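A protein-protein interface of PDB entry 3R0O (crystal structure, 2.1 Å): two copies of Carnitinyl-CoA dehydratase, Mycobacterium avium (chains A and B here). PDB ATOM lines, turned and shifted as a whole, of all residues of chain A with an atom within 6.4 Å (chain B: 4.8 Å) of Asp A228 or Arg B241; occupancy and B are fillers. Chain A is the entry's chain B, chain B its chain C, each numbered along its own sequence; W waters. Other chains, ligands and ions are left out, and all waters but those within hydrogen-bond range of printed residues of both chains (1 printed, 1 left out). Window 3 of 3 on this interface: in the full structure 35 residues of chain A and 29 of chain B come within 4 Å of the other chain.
The guanidinium group (NE) of Arg A222 lies within salt-bridge range of the side-chain carboxylate (OE2) of Glu B245, 2.6 Å away.
The guanidinium group (NH1) of Arg B241 lies within salt-bridge range of the side-chain carboxylate (OD2) of Asp A228 (2.7 Å).
NH1 of Arg B244 lies within salt-bridge range of OD1 of Asp A228 (3.2 Å).
N of Ala A227 sits at hydrogen-bond distance from O of Arg A222 (2.9 Å).
O of Lys B238 is in hydrogen-bond range of OG1 of Thr B242 (2.8 Å).
The side-chain carboxylate (OE1) of Glu B240 lies within salt-bridge range of the guanidinium group (NH1) of Arg B244 (2.8 Å).
Among the printed residues, merely in contact across the chains: Val A223 with Thr B242 (3.4 Å), Gly A226 with Arg B241 (3.6 Å), Val A223 with Glu B245 (3.8 Å), Ala A227 with Arg B241 (3.9 Å) and Arg A222 with Arg B241 (3.9 Å).
Of the printed residues of chain B, Arg A222 touches Arg B241 and Glu B245.
Printed residues of chain B within 4 Å of Val A223: Thr B242 (3.4 Å) and Glu B245 (3.8 Å).
Tyr A225 touches none of the printed residues of chain B.
Of the printed residues of chain B, Gly A226 touches Arg B241 (3.6 Å).
Of the printed residues of chain B, Ala A227 touches Arg B241.
Ile A232 touches none of the printed residues of chain B.
Arg B241 touches just these residues of chain A: Arg A222, Gly A226, Ala A227 and Asp A228.
The nearest residue of chain A that does not touch Arg B241 is Val A223 (4.04 Å).
Printed residues of chain B that touch a printed residue of chain A: Arg B241, Thr B242, Arg B244 and Glu B245.
Printed residues of chain A that touch a printed residue of chain B: Arg A222, Val A223, Gly A226, Ala A227 and Asp A228.
Hydrophobic or aromatic side chains of chain A within 4 Å of the printed part of chain B: Val A223.
Among the printed residues, Asp or Glu carboxylates within 4 Å of a Lys or Arg side-chain nitrogen of the other chain: Arg A222 with Glu B245, Asp A228 with Arg B241 and Asp A228 with Arg B244.
No position is printed for both chains.
Of the 8 pairs that touch across the chains among the printed residues, none has its exchanged pair printed and touching as well.
Water W1 lies within hydrogen-bond range of O of Val A223 (2.7 Å) and NH2 of Arg B241 (3.0 Å).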
ATOM      1  N   ARG A 222      -4.502  12.657   1.693  1.00  0.00           N
ATOM      2  CA  ARG A 222      -3.771  11.715   0.799  1.00  0.00           C
ATOM      3  C   ARG A 222      -2.815  12.424  -0.155  1.00  0.00           C
ATOM      4  O   ARG A 222      -1.645  12.049  -0.279  1.00  0.00           O
ATOM      5  CB  ARG A 222      -4.761  10.872   0.001  1.00  0.00           C
ATOM      6  CG  ARG A 222      -5.436   9.804   0.857  1.00  0.00           C
ATOM      7  CD  ARG A 222      -6.179   8.767   0.011  1.00  0.00           C
ATOM      8  NE  ARG A 222      -7.258   9.344  -0.794  1.00  0.00           N
ATOM      9  CZ  ARG A 222      -8.523   9.488  -0.400  1.00  0.00           C
ATOM     10  NH1 ARG A 222      -8.900   9.112   0.821  1.00  0.00           N
ATOM     11  NH2 ARG A 222      -9.427   9.976  -1.249  1.00  0.00           N
ATOM     12  N   VAL A 223      -3.300  13.479  -0.807  1.00  0.00           N
ATOM     13  CA  VAL A 223      -2.437  14.286  -1.701  1.00  0.00           C
ATOM     14  C   VAL A 223      -1.290  14.951  -0.924  1.00  0.00           C
ATOM     15  O   VAL A 223      -0.141  15.001  -1.412  1.00  0.00           O
ATOM     16  CB  VAL A 223      -3.260  15.368  -2.455  1.00  0.00           C
ATOM     17  CG1 VAL A 223      -2.340  16.272  -3.323  1.00  0.00           C
ATOM     18  CG2 VAL A 223      -4.353  14.701  -3.306  1.00  0.00           C
ATOM     19  N   ALA A 224      -1.595  15.475   0.265  1.00  0.00           N
ATOM     20  CA  ALA A 224      -0.583  16.213   1.047  1.00  0.00           C
ATOM     21  C   ALA A 224       0.569  15.310   1.467  1.00  0.00           C
ATOM     22  O   ALA A 224       1.710  15.754   1.496  1.00  0.00           O
ATOM     23  CB  ALA A 224      -1.201  16.912   2.266  1.00  0.00           C
ATOM     24  N   TYR A 225       0.269  14.051   1.778  1.00  0.00           N
ATOM     25  CA  TYR A 225       1.302  13.058   2.137  1.00  0.00           C
ATOM     26  C   TYR A 225       1.907  12.261   0.968  1.00  0.00           C
ATOM     27  O   TYR A 225       2.951  11.611   1.132  1.00  0.00           O
ATOM     28  CB  TYR A 225       0.757  12.092   3.197  1.00  0.00           C
ATOM     29  CG  TYR A 225       0.664  12.761   4.565  1.00  0.00           C
ATOM     30  CD1 TYR A 225       1.818  13.049   5.303  1.00  0.00           C
ATOM     31  CD2 TYR A 225      -0.574  13.122   5.107  1.00  0.00           C
ATOM     32  CE1 TYR A 225       1.747  13.664   6.576  1.00  0.00           C
ATOM     33  CE2 TYR A 225      -0.666  13.752   6.367  1.00  0.00           C
ATOM     34  CZ  TYR A 225       0.500  14.015   7.093  1.00  0.00           C
ATOM     35  OH  TYR A 225       0.419  14.629   8.327  1.00  0.00           O
ATOM     36  N   GLY A 226       1.276  12.318  -0.203  1.00  0.00           N
ATOM     37  CA  GLY A 226       1.630  11.409  -1.312  1.00  0.00           C
ATOM     38  C   GLY A 226       1.291   9.962  -0.990  1.00  0.00           C
ATOM     39  O   GLY A 226       2.056   9.054  -1.286  1.00  0.00           O
ATOM     40  N   ALA A 227       0.128   9.741  -0.384  1.00  0.00           N
ATOM     41  CA  ALA A 227      -0.296   8.382   0.004  1.00  0.00           C
ATOM     42  C   ALA A 227      -1.118   7.738  -1.105  1.00  0.00           C
ATOM     43  O   ALA A 227      -2.033   8.357  -1.628  1.00  0.00           O
ATOM     44  CB  ALA A 227      -1.103   8.435   1.314  1.00  0.00           C
ATOM     45  N   ASP A 228      -0.755   6.510  -1.479  1.00  0.00           N
ATOM     46  CA  ASP A 228      -1.496   5.696  -2.461  1.00  0.00           C
ATOM     47  C   ASP A 228      -1.796   4.356  -1.788  1.00  0.00           C
ATOM     48  O   ASP A 228      -0.894   3.735  -1.209  1.00  0.00           O
ATOM     49  CB  ASP A 228      -0.665   5.434  -3.742  1.00  0.00           C
ATOM     50  CG  ASP A 228      -0.338   6.713  -4.526  1.00  0.00           C
ATOM     51  OD1 ASP A 228      -1.211   7.604  -4.684  1.00  0.00           O
ATOM     52  OD2 ASP A 228       0.820   6.830  -4.978  1.00  0.00           O
ATOM     53  N   ASP A 229      -3.060   3.936  -1.829  1.00  0.00           N
ATOM     54  CA  ASP A 229      -3.512   2.693  -1.186  1.00  0.00           C
ATOM     55  C   ASP A 229      -3.015   2.546   0.254  1.00  0.00           C
ATOM     56  O   ASP A 229      -2.579   1.474   0.653  1.00  0.00           O
ATOM     57  CB  ASP A 229      -3.086   1.476  -2.026  1.00  0.00           C
ATOM     58  CG  ASP A 229      -3.456   1.628  -3.498  1.00  0.00           C
ATOM     59  OD1 ASP A 229      -4.655   1.822  -3.806  1.00  0.00           O
ATOM     60  OD2 ASP A 229      -2.537   1.584  -4.354  1.00  0.00           O
ATOM     61  N   GLY A 230      -3.052   3.640   1.013  1.00  0.00           N
ATOM     62  CA  GLY A 230      -2.630   3.638   2.408  1.00  0.00           C
ATOM     63  C   GLY A 230      -1.136   3.591   2.708  1.00  0.00           C
ATOM     64  O   GLY A 230      -0.749   3.376   3.853  1.00  0.00           O
ATOM     65  N   ILE A 231      -0.296   3.758   1.691  1.00  0.00           N
ATOM     66  CA  ILE A 231       1.158   3.705   1.859  1.00  0.00           C
ATOM     67  C   ILE A 231       1.732   5.029   1.407  1.00  0.00           C
ATOM     68  O   ILE A 231       1.407   5.510   0.303  1.00  0.00           O
ATOM     69  CB  ILE A 231       1.807   2.590   0.985  1.00  0.00           C
ATOM     70  CG1 ILE A 231       1.220   1.211   1.329  1.00  0.00           C
ATOM     71  CG2 ILE A 231       3.332   2.555   1.180  1.00  0.00           C
ATOM     72  CD1 ILE A 231       1.526   0.750   2.765  1.00  0.00           C
ATOM     73  N   ILE A 232       2.593   5.607   2.242  1.00  0.00           N
ATOM     74  CA  ILE A 232       3.408   6.737   1.807  1.00  0.00           C
ATOM     75  C   ILE A 232       4.696   6.173   1.189  1.00  0.00           C
ATOM     76  O   ILE A 232       5.664   5.876   1.909  1.00  0.00           O
ATOM     77  CB  ILE A 232       3.707   7.729   2.957  1.00  0.00           C
ATOM     78  CG1 ILE A 232       2.382   8.243   3.569  1.00  0.00           C
ATOM     79  CG2 ILE A 232       4.586   8.899   2.429  1.00  0.00           C
ATOM     80  CD1 ILE A 232       2.532   9.078   4.821  1.00  0.00           C
ATOM     81  N   GLY A 233       4.676   5.973  -0.127  1.00  0.00           N
ATOM     82  CA  GLY A 233       5.827   5.438  -0.881  1.00  0.00           C
ATOM     83  C   GLY A 233       7.181   6.013  -0.455  1.00  0.00           C
ATOM     84  O   GLY A 233       8.109   5.261  -0.195  1.00  0.00           O
ATOM     85  N   PRO B 237       4.340  12.848 -10.404  1.00  0.00           N
ATOM     86  CA  PRO B 237       3.409  11.925  -9.688  1.00  0.00           C
ATOM     87  C   PRO B 237       2.466  12.656  -8.716  1.00  0.00           C
ATOM     88  O   PRO B 237       1.401  12.133  -8.404  1.00  0.00           O
ATOM     89  CB  PRO B 237       4.341  10.967  -8.917  1.00  0.00           C
ATOM     90  CG  PRO B 237       5.715  11.110  -9.617  1.00  0.00           C
ATOM     91  CD  PRO B 237       5.754  12.560 -10.073  1.00  0.00           C
ATOM     92  N   LYS B 238       2.838  13.852  -8.269  1.00  0.00           N
ATOM     93  CA  LYS B 238       1.952  14.674  -7.417  1.00  0.00           C
ATOM     94  C   LYS B 238       0.775  15.244  -8.210  1.00  0.00           C
ATOM     95  O   LYS B 238      -0.368  15.262  -7.726  1.00  0.00           O
ATOM     96  CB  LYS B 238       2.747  15.797  -6.726  1.00  0.00           C
ATOM     97  CG  LYS B 238       3.815  15.258  -5.741  1.00  0.00           C
ATOM     98  CD  LYS B 238       4.621  16.376  -5.077  1.00  0.00           C
ATOM     99  CE  LYS B 238       5.891  15.836  -4.352  1.00  0.00           C
ATOM    100  NZ  LYS B 238       6.480  16.997  -3.570  1.00  0.00           N
ATOM    101  N   TRP B 239       1.054  15.745  -9.414  1.00  0.00           N
ATOM    102  CA  TRP B 239      -0.014  16.083 -10.361  1.00  0.00           C
ATOM    103  C   TRP B 239      -0.959  14.900 -10.658  1.00  0.00           C
ATOM    104  O   TRP B 239      -2.173  15.063 -10.615  1.00  0.00           O
ATOM    105  CB  TRP B 239       0.592  16.593 -11.674  1.00  0.00           C
ATOM    106  CG  TRP B 239       1.158  17.968 -11.556  1.00  0.00           C
ATOM    107  CD1 TRP B 239       2.488  18.339 -11.659  1.00  0.00           C
ATOM    108  CD2 TRP B 239       0.419  19.170 -11.312  1.00  0.00           C
ATOM    109  NE1 TRP B 239       2.603  19.692 -11.505  1.00  0.00           N
ATOM    110  CE2 TRP B 239       1.353  20.234 -11.298  1.00  0.00           C
ATOM    111  CE3 TRP B 239      -0.952  19.457 -11.125  1.00  0.00           C
ATOM    112  CZ2 TRP B 239       0.970  21.572 -11.074  1.00  0.00           C
ATOM    113  CZ3 TRP B 239      -1.340  20.808 -10.903  1.00  0.00           C
ATOM    114  CH2 TRP B 239      -0.381  21.832 -10.874  1.00  0.00           C
ATOM    115  N   GLU B 240      -0.403  13.717 -10.948  1.00  0.00           N
ATOM    116  CA  GLU B 240      -1.234  12.542 -11.282  1.00  0.00           C
ATOM    117  C   GLU B 240      -2.204  12.229 -10.125  1.00  0.00           C
ATOM    118  O   GLU B 240      -3.397  11.995 -10.343  1.00  0.00           O
ATOM    119  CB  GLU B 240      -0.367  11.306 -11.611  1.00  0.00           C
ATOM    120  CG  GLU B 240      -1.099  10.086 -12.175  1.00  0.00           C
ATOM    121  CD  GLU B 240      -1.948   9.278 -11.155  1.00  0.00           C
ATOM    122  OE1 GLU B 240      -1.617   9.248  -9.930  1.00  0.00           O
ATOM    123  OE2 GLU B 240      -2.951   8.633 -11.600  1.00  0.00           O
ATOM    124  N   ARG B 241      -1.660  12.210  -8.909  1.00  0.00           N
ATOM    125  CA  ARG B 241      -2.416  11.950  -7.685  1.00  0.00           C
ATOM    126  C   ARG B 241      -3.504  12.983  -7.481  1.00  0.00           C
ATOM    127  O   ARG B 241      -4.655  12.633  -7.267  1.00  0.00           O
ATOM    128  CB  ARG B 241      -1.458  11.962  -6.488  1.00  0.00           C
ATOM    129  CG  ARG B 241      -2.080  11.479  -5.207  1.00  0.00           C
ATOM    130  CD  ARG B 241      -1.015  11.372  -4.109  1.00  0.00           C
ATOM    131  NE  ARG B 241      -0.112  10.271  -4.422  1.00  0.00           N
ATOM    132  CZ  ARG B 241       1.158  10.394  -4.781  1.00  0.00           C
ATOM    133  NH1 ARG B 241       1.857   9.300  -5.065  1.00  0.00           N
ATOM    134  NH2 ARG B 241       1.736  11.590  -4.857  1.00  0.00           N
ATOM    135  N   THR B 242      -3.140  14.252  -7.563  1.00  0.00           N
ATOM    136  CA  THR B 242      -4.103  15.358  -7.464  1.00  0.00           C
ATOM    137  C   THR B 242      -5.276  15.219  -8.447  1.00  0.00           C
ATOM    138  O   THR B 242      -6.446  15.284  -8.050  1.00  0.00           O
ATOM    139  CB  THR B 242      -3.393  16.703  -7.686  1.00  0.00           C
ATOM    140  OG1 THR B 242      -2.435  16.871  -6.654  1.00  0.00           O
ATOM    141  CG2 THR B 242      -4.357  17.889  -7.653  1.00  0.00           C
ATOM    142  N   ILE B 243      -4.959  15.007  -9.727  1.00  0.00           N
ATOM    143  CA  ILE B 243      -6.006  14.914 -10.755  1.00  0.00           C
ATOM    144  C   ILE B 243      -6.921  13.698 -10.518  1.00  0.00           C
ATOM    145  O   ILE B 243      -8.151  13.790 -10.641  1.00  0.00           O
ATOM    146  CB  ILE B 243      -5.390  14.928 -12.177  1.00  0.00           C
ATOM    147  CG1 ILE B 243      -4.675  16.278 -12.434  1.00  0.00           C
ATOM    148  CG2 ILE B 243      -6.477  14.684 -13.279  1.00  0.00           C
ATOM    149  CD1 ILE B 243      -3.599  16.205 -13.555  1.00  0.00           C
ATOM    150  N   ARG B 244      -6.320  12.551 -10.189  1.00  0.00           N
ATOM    151  CA  ARG B 244      -7.109  11.349  -9.883  1.00  0.00           C
ATOM    152  C   ARG B 244      -8.102  11.603  -8.722  1.00  0.00           C
ATOM    153  O   ARG B 244      -9.295  11.279  -8.817  1.00  0.00           O
ATOM    154  CB  ARG B 244      -6.150  10.202  -9.557  1.00  0.00           C
ATOM    155  CG  ARG B 244      -6.780   8.904  -9.168  1.00  0.00           C
ATOM    156  CD  ARG B 244      -5.774   7.742  -9.266  1.00  0.00           C
ATOM    157  NE  ARG B 244      -4.387   8.090  -8.899  1.00  0.00           N
ATOM    158  CZ  ARG B 244      -3.886   8.021  -7.664  1.00  0.00           C
ATOM    159  NH1 ARG B 244      -2.612   8.331  -7.443  1.00  0.00           N
ATOM    160  NH2 ARG B 244      -4.644   7.646  -6.640  1.00  0.00           N
ATOM    161  N   GLU B 245      -7.595  12.183  -7.627  1.00  0.00           N
ATOM    162  CA  GLU B 245      -8.399  12.492  -6.468  1.00  0.00           C
ATOM    163  C   GLU B 245      -9.492  13.509  -6.814  1.00  0.00           C
ATOM    164  O   GLU B 245     -10.646  13.372  -6.392  1.00  0.00           O
ATOM    165  CB  GLU B 245      -7.518  13.018  -5.316  1.00  0.00           C
ATOM    166  CG  GLU B 245      -6.537  11.969  -4.691  1.00  0.00           C
ATOM    167  CD  GLU B 245      -7.168  11.026  -3.697  1.00  0.00           C
ATOM    168  OE1 GLU B 245      -8.391  11.142  -3.434  1.00  0.00           O
ATOM    169  OE2 GLU B 245      -6.441  10.143  -3.165  1.00  0.00           O
HETATM  170  O   HOH W   1       1.275  14.215  -3.568  1.00  0.00           O
